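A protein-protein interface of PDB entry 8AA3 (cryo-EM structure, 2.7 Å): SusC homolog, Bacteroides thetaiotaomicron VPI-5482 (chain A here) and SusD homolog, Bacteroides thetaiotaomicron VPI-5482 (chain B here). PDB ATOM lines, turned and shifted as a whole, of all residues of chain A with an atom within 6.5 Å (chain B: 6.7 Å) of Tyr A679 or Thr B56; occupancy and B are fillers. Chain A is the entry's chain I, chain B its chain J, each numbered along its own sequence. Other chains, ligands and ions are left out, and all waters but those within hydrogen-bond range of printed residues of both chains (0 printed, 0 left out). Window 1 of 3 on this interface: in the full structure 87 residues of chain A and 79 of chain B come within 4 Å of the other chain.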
ATOM      1  N   ASN A 667      30.317  -1.436  24.548  1.00  0.00           N
ATOM      2  CA  ASN A 667      31.088  -0.671  23.571  1.00  0.00           C
ATOM      3  C   ASN A 667      31.007   0.803  23.946  1.00  0.00           C
ATOM      4  O   ASN A 667      30.097   1.525  23.537  1.00  0.00           O
ATOM      5  CB  ASN A 667      30.570  -0.921  22.160  1.00  0.00           C
ATOM      6  CG  ASN A 667      31.358  -0.168  21.107  1.00  0.00           C
ATOM      7  OD1 ASN A 667      30.793   0.346  20.142  1.00  0.00           O
ATOM      8  ND2 ASN A 667      32.671  -0.098  21.289  1.00  0.00           N
ATOM      9  N   TYR A 668      31.976   1.252  24.747  1.00  0.00           N
ATOM     10  CA  TYR A 668      31.996   2.646  25.180  1.00  0.00           C
ATOM     11  C   TYR A 668      32.202   3.588  24.001  1.00  0.00           C
ATOM     12  O   TYR A 668      31.588   4.659  23.937  1.00  0.00           O
ATOM     13  CB  TYR A 668      33.087   2.849  26.232  1.00  0.00           C
ATOM     14  CG  TYR A 668      33.071   4.213  26.888  1.00  0.00           C
ATOM     15  CD1 TYR A 668      32.297   4.450  28.017  1.00  0.00           C
ATOM     16  CD2 TYR A 668      33.837   5.257  26.387  1.00  0.00           C
ATOM     17  CE1 TYR A 668      32.280   5.692  28.623  1.00  0.00           C
ATOM     18  CE2 TYR A 668      33.826   6.502  26.987  1.00  0.00           C
ATOM     19  CZ  TYR A 668      33.047   6.714  28.105  1.00  0.00           C
ATOM     20  OH  TYR A 668      33.033   7.952  28.705  1.00  0.00           O
ATOM     21  N   GLY A 669      33.059   3.207  23.057  1.00  0.00           N
ATOM     22  CA  GLY A 669      33.327   4.036  21.899  1.00  0.00           C
ATOM     23  C   GLY A 669      34.781   4.438  21.786  1.00  0.00           C
ATOM     24  O   GLY A 669      35.108   5.456  21.168  1.00  0.00           O
ATOM     25  N   SER A 673      36.741   4.597  14.297  1.00  0.00           N
ATOM     26  CA  SER A 673      35.771   4.271  13.263  1.00  0.00           C
ATOM     27  C   SER A 673      35.805   5.346  12.187  1.00  0.00           C
ATOM     28  O   SER A 673      36.098   6.512  12.461  1.00  0.00           O
ATOM     29  CB  SER A 673      34.354   4.143  13.836  1.00  0.00           C
ATOM     30  OG  SER A 673      33.415   3.856  12.815  1.00  0.00           O
ATOM     31  N   GLY A 676      32.150   8.016  11.528  1.00  0.00           N
ATOM     32  CA  GLY A 676      31.435   8.268  12.759  1.00  0.00           C
ATOM     33  C   GLY A 676      30.450   7.197  13.174  1.00  0.00           C
ATOM     34  O   GLY A 676      29.761   7.375  14.187  1.00  0.00           O
ATOM     35  N   GLN A 677      30.356   6.097  12.434  1.00  0.00           N
ATOM     36  CA  GLN A 677      29.447   5.005  12.781  1.00  0.00           C
ATOM     37  C   GLN A 677      30.099   4.025  13.752  1.00  0.00           C
ATOM     38  O   GLN A 677      30.141   2.818  13.521  1.00  0.00           O
ATOM     39  CB  GLN A 677      28.980   4.296  11.516  1.00  0.00           C
ATOM     40  CG  GLN A 677      30.088   4.005  10.518  1.00  0.00           C
ATOM     41  CD  GLN A 677      29.622   3.131   9.371  1.00  0.00           C
ATOM     42  OE1 GLN A 677      28.803   2.230   9.555  1.00  0.00           O
ATOM     43  NE2 GLN A 677      30.143   3.393   8.178  1.00  0.00           N
ATOM     44  N   SER A 678      30.614   4.553  14.865  1.00  0.00           N
ATOM     45  CA  SER A 678      31.273   3.711  15.855  1.00  0.00           C
ATOM     46  C   SER A 678      30.288   2.856  16.638  1.00  0.00           C
ATOM     47  O   SER A 678      30.689   1.827  17.194  1.00  0.00           O
ATOM     48  CB  SER A 678      32.091   4.573  16.819  1.00  0.00           C
ATOM     49  OG  SER A 678      31.249   5.249  17.737  1.00  0.00           O
ATOM     50  N   TYR A 679      29.016   3.260  16.698  1.00  0.00           N
ATOM     51  CA  TYR A 679      27.981   2.544  17.446  1.00  0.00           C
ATOM     52  C   TYR A 679      28.351   2.395  18.919  1.00  0.00           C
ATOM     53  O   TYR A 679      27.948   1.432  19.578  1.00  0.00           O
ATOM     54  CB  TYR A 679      27.689   1.174  16.826  1.00  0.00           C
ATOM     55  CG  TYR A 679      26.854   1.233  15.567  1.00  0.00           C
ATOM     56  CD1 TYR A 679      25.497   1.528  15.623  1.00  0.00           C
ATOM     57  CD2 TYR A 679      27.421   0.994  14.321  1.00  0.00           C
ATOM     58  CE1 TYR A 679      24.731   1.583  14.475  1.00  0.00           C
ATOM     59  CE2 TYR A 679      26.661   1.047  13.169  1.00  0.00           C
ATOM     60  CZ  TYR A 679      25.317   1.342  13.252  1.00  0.00           C
ATOM     61  OH  TYR A 679      24.557   1.396  12.106  1.00  0.00           O
ATOM     62  N   GLY A 680      29.119   3.344  19.446  1.00  0.00           N
ATOM     63  CA  GLY A 680      29.505   3.289  20.839  1.00  0.00           C
ATOM     64  C   GLY A 680      28.354   3.622  21.768  1.00  0.00           C
ATOM     65  O   GLY A 680      27.327   4.173  21.369  1.00  0.00           O
ATOM     66  N   THR A 681      28.535   3.276  23.039  1.00  0.00           N
ATOM     67  CA  THR A 681      27.523   3.501  24.067  1.00  0.00           C
ATOM     68  C   THR A 681      28.105   4.467  25.096  1.00  0.00           C
ATOM     69  O   THR A 681      28.680   4.052  26.106  1.00  0.00           O
ATOM     70  CB  THR A 681      27.085   2.189  24.708  1.00  0.00           C
ATOM     71  OG1 THR A 681      26.635   1.287  23.690  1.00  0.00           O
ATOM     72  CG2 THR A 681      25.946   2.439  25.675  1.00  0.00           C
ATOM     73  N   ALA A 682      27.952   5.762  24.829  1.00  0.00           N
ATOM     74  CA  ALA A 682      28.408   6.807  25.743  1.00  0.00           C
ATOM     75  C   ALA A 682      27.686   8.091  25.373  1.00  0.00           C
ATOM     76  O   ALA A 682      27.872   8.605  24.266  1.00  0.00           O
ATOM     77  CB  ALA A 682      29.923   6.989  25.663  1.00  0.00           C
ATOM     78  N   LYS A 699      25.253  -2.944  24.361  1.00  0.00           N
ATOM     79  CA  LYS A 699      24.579  -3.079  23.079  1.00  0.00           C
ATOM     80  C   LYS A 699      24.611  -4.537  22.646  1.00  0.00           C
ATOM     81  O   LYS A 699      25.519  -5.289  23.010  1.00  0.00           O
ATOM     82  CB  LYS A 699      25.221  -2.194  22.000  1.00  0.00           C
ATOM     83  CG  LYS A 699      26.534  -2.725  21.445  1.00  0.00           C
ATOM     84  CD  LYS A 699      27.063  -1.831  20.335  1.00  0.00           C
ATOM     85  CE  LYS A 699      28.331  -2.400  19.720  1.00  0.00           C
ATOM     86  NZ  LYS A 699      28.065  -3.660  18.973  1.00  0.00           N
ATOM     87  N   GLU A 755      20.141  -3.716  15.383  1.00  0.00           N
ATOM     88  CA  GLU A 755      21.473  -4.238  15.643  1.00  0.00           C
ATOM     89  C   GLU A 755      21.393  -5.575  16.372  1.00  0.00           C
ATOM     90  O   GLU A 755      20.467  -5.835  17.144  1.00  0.00           O
ATOM     91  CB  GLU A 755      22.291  -3.240  16.462  1.00  0.00           C
ATOM     92  CG  GLU A 755      21.795  -3.046  17.884  1.00  0.00           C
ATOM     93  CD  GLU A 755      22.644  -2.068  18.670  1.00  0.00           C
ATOM     94  OE1 GLU A 755      23.588  -1.494  18.087  1.00  0.00           O
ATOM     95  OE2 GLU A 755      22.370  -1.879  19.873  1.00  0.00           O
ATOM     96  N   SER B  49      22.214   3.507  26.635  1.00  0.00           N
ATOM     97  CA  SER B  49      22.353   2.997  25.276  1.00  0.00           C
ATOM     98  C   SER B  49      21.330   3.640  24.351  1.00  0.00           C
ATOM     99  O   SER B  49      21.670   4.106  23.256  1.00  0.00           O
ATOM    100  CB  SER B  49      22.205   1.476  25.270  1.00  0.00           C
ATOM    101  OG  SER B  49      23.157   0.862  26.122  1.00  0.00           O
ATOM    102  N   TYR B  51      20.111   6.435  24.364  1.00  0.00           N
ATOM    103  CA  TYR B  51      20.515   7.783  23.994  1.00  0.00           C
ATOM    104  C   TYR B  51      21.759   7.780  23.116  1.00  0.00           C
ATOM    105  O   TYR B  51      21.861   8.584  22.181  1.00  0.00           O
ATOM    106  CB  TYR B  51      20.765   8.621  25.251  1.00  0.00           C
ATOM    107  CG  TYR B  51      19.503   9.018  25.983  1.00  0.00           C
ATOM    108  CD1 TYR B  51      18.704  10.054  25.518  1.00  0.00           C
ATOM    109  CD2 TYR B  51      19.112   8.356  27.139  1.00  0.00           C
ATOM    110  CE1 TYR B  51      17.550  10.420  26.185  1.00  0.00           C
ATOM    111  CE2 TYR B  51      17.960   8.713  27.812  1.00  0.00           C
ATOM    112  CZ  TYR B  51      17.183   9.746  27.331  1.00  0.00           C
ATOM    113  OH  TYR B  51      16.036  10.105  28.000  1.00  0.00           O
ATOM    114  N   ALA B  52      22.695   6.864  23.385  1.00  0.00           N
ATOM    115  CA  ALA B  52      23.983   6.896  22.701  1.00  0.00           C
ATOM    116  C   ALA B  52      23.834   6.680  21.203  1.00  0.00           C
ATOM    117  O   ALA B  52      24.615   7.227  20.416  1.00  0.00           O
ATOM    118  CB  ALA B  52      24.919   5.846  23.296  1.00  0.00           C
ATOM    119  N   ILE B  53      22.832   5.899  20.788  1.00  0.00           N
ATOM    120  CA  ILE B  53      22.628   5.644  19.367  1.00  0.00           C
ATOM    121  C   ILE B  53      22.302   6.933  18.627  1.00  0.00           C
ATOM    122  O   ILE B  53      22.556   7.045  17.422  1.00  0.00           O
ATOM    123  CB  ILE B  53      21.530   4.582  19.167  1.00  0.00           C
ATOM    124  CG1 ILE B  53      21.650   3.936  17.784  1.00  0.00           C
ATOM    125  CG2 ILE B  53      20.143   5.177  19.379  1.00  0.00           C
ATOM    126  CD1 ILE B  53      22.995   3.295  17.529  1.00  0.00           C
ATOM    127  N   TRP B  54      21.751   7.927  19.326  1.00  0.00           N
ATOM    128  CA  TRP B  54      21.442   9.197  18.686  1.00  0.00           C
ATOM    129  C   TRP B  54      22.665  10.088  18.530  1.00  0.00           C
ATOM    130  O   TRP B  54      22.575  11.125  17.863  1.00  0.00           O
ATOM    131  CB  TRP B  54      20.355   9.932  19.476  1.00  0.00           C
ATOM    132  CG  TRP B  54      19.028   9.236  19.427  1.00  0.00           C
ATOM    133  CD1 TRP B  54      18.433   8.531  20.433  1.00  0.00           C
ATOM    134  CD2 TRP B  54      18.137   9.162  18.306  1.00  0.00           C
ATOM    135  NE1 TRP B  54      17.225   8.032  20.011  1.00  0.00           N
ATOM    136  CE2 TRP B  54      17.020   8.404  18.709  1.00  0.00           C
ATOM    137  CE3 TRP B  54      18.175   9.667  17.003  1.00  0.00           C
ATOM    138  CZ2 TRP B  54      15.951   8.139  17.856  1.00  0.00           C
ATOM    139  CZ3 TRP B  54      17.113   9.402  16.157  1.00  0.00           C
ATOM    140  CH2 TRP B  54      16.016   8.645  16.587  1.00  0.00           C
ATOM    141  N   ALA B  55      23.801   9.711  19.120  1.00  0.00           N
ATOM    142  CA  ALA B  55      25.040  10.458  18.970  1.00  0.00           C
ATOM    143  C   ALA B  55      26.168   9.662  18.333  1.00  0.00           C
ATOM    144  O   ALA B  55      27.117  10.272  17.828  1.00  0.00           O
ATOM    145  CB  ALA B  55      25.520  10.985  20.332  1.00  0.00           C
ATOM    146  N   THR B  56      26.097   8.330  18.337  1.00  0.00           N
ATOM    147  CA  THR B  56      27.137   7.491  17.761  1.00  0.00           C
ATOM    148  C   THR B  56      26.632   6.586  16.646  1.00  0.00           C
ATOM    149  O   THR B  56      27.442   5.904  16.009  1.00  0.00           O
ATOM    150  CB  THR B  56      27.792   6.626  18.848  1.00  0.00           C
ATOM    151  OG1 THR B  56      26.827   5.705  19.373  1.00  0.00           O
ATOM    152  CG2 THR B  56      28.319   7.495  19.976  1.00  0.00           C
ATOM    153  N   GLY B  57      25.327   6.558  16.393  1.00  0.00           N
ATOM    154  CA  GLY B  57      24.771   5.669  15.391  1.00  0.00           C
ATOM    155  C   GLY B  57      24.464   6.340  14.070  1.00  0.00           C
ATOM    156  O   GLY B  57      23.692   5.810  13.267  1.00  0.00           O
ATOM    157  N   ASP B  58      25.055   7.508  13.832  1.00  0.00           N
ATOM    158  CA  ASP B  58      24.835   8.264  12.607  1.00  0.00           C
ATOM    159  C   ASP B  58      26.125   8.334  11.802  1.00  0.00           C
ATOM    160  O   ASP B  58      27.208   8.532  12.362  1.00  0.00           O
ATOM    161  CB  ASP B  58      24.325   9.678  12.913  1.00  0.00           C
ATOM    162  CG  ASP B  58      25.289  10.473  13.771  1.00  0.00           C
ATOM    163  OD1 ASP B  58      25.639   9.996  14.871  1.00  0.00           O
ATOM    164  OD2 ASP B  58      25.697  11.573  13.346  1.00  0.00           O
ATOM    165  N   ASP B  59      26.002   8.167  10.490  1.00  0.00           N
ATOM    166  CA  ASP B  59      27.132   8.213   9.576  1.00  0.00           C
ATOM    167  C   ASP B  59      27.150   9.541   8.823  1.00  0.00           C
ATOM    168  O   ASP B  59      26.230  10.356   8.922  1.00  0.00           O
ATOM    169  CB  ASP B  59      27.072   7.036   8.595  1.00  0.00           C
ATOM    170  CG  ASP B  59      28.420   6.721   7.975  1.00  0.00           C
ATOM    171  OD1 ASP B  59      29.411   6.615   8.726  1.00  0.00           O
ATOM    172  OD2 ASP B  59      28.488   6.579   6.736  1.00  0.00           O
ATOM    173  N   PHE B  64      20.906  11.559  11.378  1.00  0.00           N
ATOM    174  CA  PHE B  64      19.556  11.657  11.917  1.00  0.00           C
ATOM    175  C   PHE B  64      18.945  13.039  11.729  1.00  0.00           C
ATOM    176  O   PHE B  64      17.733  13.191  11.914  1.00  0.00           O
ATOM    177  CB  PHE B  64      19.564  11.277  13.398  1.00  0.00           C
ATOM    178  CG  PHE B  64      20.032   9.874  13.651  1.00  0.00           C
ATOM    179  CD1 PHE B  64      19.677   8.848  12.790  1.00  0.00           C
ATOM    180  CD2 PHE B  64      20.837   9.582  14.737  1.00  0.00           C
ATOM    181  CE1 PHE B  64      20.110   7.556  13.013  1.00  0.00           C
ATOM    182  CE2 PHE B  64      21.272   8.291  14.965  1.00  0.00           C
ATOM    183  CZ  PHE B  64      20.908   7.277  14.102  1.00  0.00           C
ATOM    184  N   ASP B 107      20.468   2.012   4.250  1.00  0.00           N
ATOM    185  CA  ASP B 107      21.310   2.355   5.390  1.00  0.00           C
ATOM    186  C   ASP B 107      20.533   3.150   6.431  1.00  0.00           C
ATOM    187  O   ASP B 107      20.580   2.838   7.626  1.00  0.00           O
ATOM    188  CB  ASP B 107      22.536   3.137   4.916  1.00  0.00           C
ATOM    189  CG  ASP B 107      23.702   3.031   5.879  1.00  0.00           C
ATOM    190  OD1 ASP B 107      23.939   1.925   6.408  1.00  0.00           O
ATOM    191  OD2 ASP B 107      24.382   4.055   6.105  1.00  0.00           O
ATOM    192  N   LYS B 110      17.962   0.939   8.159  1.00  0.00           N
ATOM    193  CA  LYS B 110      18.572   0.049   9.139  1.00  0.00           C
ATOM    194  C   LYS B 110      19.008   0.807  10.386  1.00  0.00           C
ATOM    195  O   LYS B 110      18.842   0.312  11.502  1.00  0.00           O
ATOM    196  CB  LYS B 110      19.757  -0.683   8.511  1.00  0.00           C
ATOM    197  CG  LYS B 110      19.359  -1.786   7.542  1.00  0.00           C
ATOM    198  CD  LYS B 110      20.536  -2.691   7.222  1.00  0.00           C
ATOM    199  CE  LYS B 110      21.575  -1.967   6.380  1.00  0.00           C
ATOM    200  NZ  LYS B 110      22.582  -2.904   5.811  1.00  0.00           N
ATOM    201  N   ARG B 111      19.573   2.005  10.219  1.00  0.00           N
ATOM    202  CA  ARG B 111      20.030   2.767  11.380  1.00  0.00           C
ATOM    203  C   ARG B 111      18.861   3.198  12.260  1.00  0.00           C
ATOM    204  O   ARG B 111      18.927   3.089  13.494  1.00  0.00           O
ATOM    205  CB  ARG B 111      20.842   3.980  10.925  1.00  0.00           C
ATOM    206  CG  ARG B 111      22.100   3.619  10.152  1.00  0.00           C
ATOM    207  CD  ARG B 111      23.222   4.611  10.382  1.00  0.00           C
ATOM    208  NE  ARG B 111      24.305   4.427   9.423  1.00  0.00           N
ATOM    209  CZ  ARG B 111      25.478   3.880   9.712  1.00  0.00           C
ATOM    210  NH1 ARG B 111      25.760   3.457  10.934  1.00  0.00           N
ATOM    211  NH2 ARG B 111      26.390   3.753   8.753  1.00  0.00           N
ATOM    212  N   GLN B 114      17.639   0.264  14.070  1.00  0.00           N
ATOM    213  CA  GLN B 114      18.557  -0.045  15.164  1.00  0.00           C
ATOM    214  C   GLN B 114      18.270   0.829  16.379  1.00  0.00           C
ATOM    215  O   GLN B 114      18.306   0.354  17.522  1.00  0.00           O
ATOM    216  CB  GLN B 114      20.004   0.140  14.704  1.00  0.00           C
ATOM    217  CG  GLN B 114      20.523  -0.966  13.802  1.00  0.00           C
ATOM    218  CD  GLN B 114      21.866  -0.631  13.184  1.00  0.00           C
ATOM    219  OE1 GLN B 114      21.938   0.055  12.164  1.00  0.00           O
ATOM    220  NE2 GLN B 114      22.938  -1.117  13.799  1.00  0.00           N
ATOM    221  N   ARG B 118      17.132  -0.554  20.056  1.00  0.00           N
ATOM    222  CA  ARG B 118      17.704  -0.172  21.346  1.00  0.00           C
ATOM    223  C   ARG B 118      16.628   0.344  22.292  1.00  0.00           C
ATOM    224  O   ARG B 118      16.607  -0.012  23.480  1.00  0.00           O
ATOM    225  CB  ARG B 118      18.792   0.884  21.157  1.00  0.00           C
ATOM    226  CG  ARG B 118      20.136   0.348  20.696  1.00  0.00           C
ATOM    227  CD  ARG B 118      21.147   1.476  20.659  1.00  0.00           C
ATOM    228  NE  ARG B 118      22.438   1.085  20.106  1.00  0.00           N
ATOM    229  CZ  ARG B 118      23.501   0.768  20.831  1.00  0.00           C
ATOM    230  NH1 ARG B 118      23.460   0.767  22.153  1.00  0.00           N
ATOM    231  NH2 ARG B 118      24.635   0.452  20.214  1.00  0.00           N
ATOM    232  N   TYR B 291      26.122  16.475  22.166  1.00  0.00           N
ATOM    233  CA  TYR B 291      27.406  16.095  21.596  1.00  0.00           C
ATOM    234  C   TYR B 291      28.516  16.609  22.502  1.00  0.00           C
ATOM    235  O   TYR B 291      28.495  17.772  22.918  1.00  0.00           O
ATOM    236  CB  TYR B 291      27.563  16.652  20.181  1.00  0.00           C
ATOM    237  CG  TYR B 291      26.665  15.987  19.159  1.00  0.00           C
ATOM    238  CD1 TYR B 291      26.905  14.687  18.737  1.00  0.00           C
ATOM    239  CD2 TYR B 291      25.575  16.659  18.622  1.00  0.00           C
ATOM    240  CE1 TYR B 291      26.088  14.075  17.805  1.00  0.00           C
ATOM    241  CE2 TYR B 291      24.751  16.055  17.690  1.00  0.00           C
ATOM    242  CZ  TYR B 291      25.012  14.763  17.286  1.00  0.00           C
ATOM    243  OH  TYR B 291      24.196  14.158  16.358  1.00  0.00           O
ATOM    244  N   GLY B 300      35.722  11.723  20.901  1.00  0.00           N
ATOM    245  CA  GLY B 300      34.570  12.457  21.401  1.00  0.00           C
ATOM    246  C   GLY B 300      33.311  12.146  20.620  1.00  0.00           C
ATOM    247  O   GLY B 300      33.340  11.796  19.441  1.00  0.00           O
ATOM    248  N   ASN B 301      32.171  12.279  21.300  1.00  0.00           N
ATOM    249  CA  ASN B 301      30.869  12.064  20.666  1.00  0.00           C
ATOM    250  C   ASN B 301      30.496  13.311  19.864  1.00  0.00           C
ATOM    251  O   ASN B 301      29.567  14.055  20.184  1.00  0.00           O
ATOM    252  CB  ASN B 301      29.809  11.725  21.705  1.00  0.00           C
ATOM    253  CG  ASN B 301      30.094  10.423  22.426  1.00  0.00           C
ATOM    254  OD1 ASN B 301      30.023  10.350  23.653  1.00  0.00           O
ATOM    255  ND2 ASN B 301      30.428   9.387  21.667  1.00  0.00           N
ATOM    256  N   LEU B 302      31.259  13.534  18.798  1.00  0.00           N
ATOM    257  CA  LEU B 302      31.053  14.684  17.936  1.00  0.00           C
ATOM    258  C   LEU B 302      29.923  14.416  16.946  1.00  0.00           C
ATOM    259  O   LEU B 302      29.484  13.280  16.748  1.00  0.00           O
ATOM    260  CB  LEU B 302      32.342  15.031  17.193  1.00  0.00           C
ATOM    261  CG  LEU B 302      33.603  15.146  18.052  1.00  0.00           C
ATOM    262  CD1 LEU B 302      34.820  15.423  17.184  1.00  0.00           C
ATOM    263  CD2 LEU B 302      33.434  16.226  19.107  1.00  0.00           C
ATOM    264  N   TRP B 304      29.247  13.671  13.862  1.00  0.00           N
ATOM    265  CA  TRP B 304      29.848  13.135  12.647  1.00  0.00           C
ATOM    266  C   TRP B 304      28.917  13.230  11.446  1.00  0.00           C
ATOM    267  O   TRP B 304      29.379  13.094  10.308  1.00  0.00           O
ATOM    268  CB  TRP B 304      30.274  11.683  12.865  1.00  0.00           C
ATOM    269  CG  TRP B 304      31.216  11.503  14.017  1.00  0.00           C
ATOM    270  CD1 TRP B 304      30.929  10.955  15.233  1.00  0.00           C
ATOM    271  CD2 TRP B 304      32.600  11.872  14.059  1.00  0.00           C
ATOM    272  NE1 TRP B 304      32.048  10.961  16.030  1.00  0.00           N
ATOM    273  CE2 TRP B 304      33.087  11.518  15.332  1.00  0.00           C
ATOM    274  CE3 TRP B 304      33.472  12.467  13.143  1.00  0.00           C
ATOM    275  CZ2 TRP B 304      34.409  11.740  15.713  1.00  0.00           C
ATOM    276  CZ3 TRP B 304      34.784  12.687  13.524  1.00  0.00           C
ATOM    277  CH2 TRP B 304      35.239  12.324  14.797  1.00  0.00           C
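The side-chain hydroxyl (OH) of Tyr A679 sits at hydrogen-bond distance from the guanidinium group (NH1) of Arg B111, at 2.7 Å.
The side-chain carboxylate (OD1) of Asp B59 lies close to the side-chain amide nitrogen (NE2) of Gln A677 (3.3 Å).
The side-chain amide oxygen (OE1) of Gln A677 is in hydrogen-bond range of the guanidinium group (NH2) of Arg B111 (3.0 Å).
The side-chain hydroxyl (OH) of Tyr A679 sits at hydrogen-bond distance from the side-chain amide oxygen (OE1) of Gln B114 (2.9 Å).
The backbone carbonyl oxygen (O) of Asp B58 sits close to the backbone carbonyl oxygen (O) of Gly A676 (3.3 Å).
The side-chain amide oxygen (OD1) of Asn B301 lies close to the backbone carbonyl oxygen (O) of Ala A682 (2.8 Å).
The backbone carbonyl oxygen (O) of Gly A680 is in hydrogen-bond range of the side-chain hydroxyl (OG1) of Thr B56.
OE2 of Glu A755 is in salt-bridge range of NE of Arg B118 (3.0 Å).
O of Thr B56 sits at hydrogen-bond distance from N of Tyr A679, at 3.2 Å.
The backbone carbonyl oxygen of Thr B56 lies close to the backbone carbonyl oxygen of Gly A676, at 3.3 Å.
The side-chain amide oxygen (OE1) of Gln B114 sits close to the backbone carbonyl oxygen (O) of Lys B110.
O of Asn A667 sits close to OG1 of Thr A681 (3.5 Å).
O of Ser A678 sits close to OD1 of Asn A667 (3.3 Å).
OD2 of Asp B107 is in salt-bridge range of NH2 of Arg B111.
O of Tyr A679 lies close to OD1 of Asn A667 (3.1 Å).
The backbone carbonyl oxygen of Ala B52 lies within hydrogen-bond range of the side-chain hydroxyl of Thr B56, at 2.9 Å.
Among the printed residues, pairs that only touch across the chains: Gly A676 with Trp B304 (3.5 Å), Gln A677 with Thr B56 (3.9 Å), Gln A677 with Asp B58 (3.98 Å), Ser A678 with Thr B56 (3.6 Å), Tyr A679 with Ile B53 (3.6 Å), Tyr A679 with Arg B118 (3.5 Å), Gly A680 with Ala B52 (3.5 Å), Thr A681 with Ser B49 (3.2 Å), Thr A681 with Ala B52 (3.6 Å), Thr A681 with Arg B118 (3.6 Å), Ala A682 with Ala B52 (3.4 Å), Lys A699 with Arg B118 (3.2 Å) and Glu A755 with Gln B114 (3.2 Å).
Of chain B, only Ile B53 (3.6 Å), Thr B56 (3.2 Å), Arg B111 (2.7 Å), Gln B114 (2.9 Å) and Arg B118 (3.5 Å) come within 4 Å of Tyr A679.
Of chain A, only Gly A676, Gln A677, Ser A678, Tyr A679 and Gly A680 come within 4 Å of Thr B56.
Of the printed residues of chain A, Asp B58 touches Gly A676 and Gln A677.
Printed residues of chain A within 4 Å of Ala B52: Gly A680 (3.5 Å), Thr A681 (3.6 Å) and Ala A682 (3.4 Å).
Of the printed residues of chain A, Arg B111 touches Gln A677 (3.0 Å) and Tyr A679 (2.7 Å).
Of the printed residues of chain B, Thr A681 touches Ser B49 (3.2 Å), Ala B52 (3.6 Å) and Arg B118 (3.6 Å).
Of the printed residues of chain A, Ile B53 touches Tyr A679 (3.6 Å).
Phe B64 touches none of the printed residues of chain A.
Gly A669 touches none of the printed residues of chain B.
The nearest residue of chain B that does not touch Tyr A679 is Gly B57 (4.2 Å).
The nearest residue of chain A that does not touch Thr B56 is Ala A682 (4.5 Å).
Hydrophobic or aromatic side chains of chain B within 4 Å of the printed part of chain A: Ala B52, Ile B53 and Trp B304.
Of the 13 printed residues of chain A, 9 touch a printed residue of chain B.
Hydrophobic or aromatic side chains of chain A within 4 Å of the printed part of chain B: Tyr A679 and Ala A682.
Along chain A the printed residues that touch a printed residue of chain B span positions 676 to 755.
Among the printed residues, 23 pairs touch across the chains.
Among the printed residues, Asp or Glu carboxylates within 4 Å of a Lys or Arg side-chain nitrogen of the other chain: Glu A755 with Arg B118 (3.0 Å).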
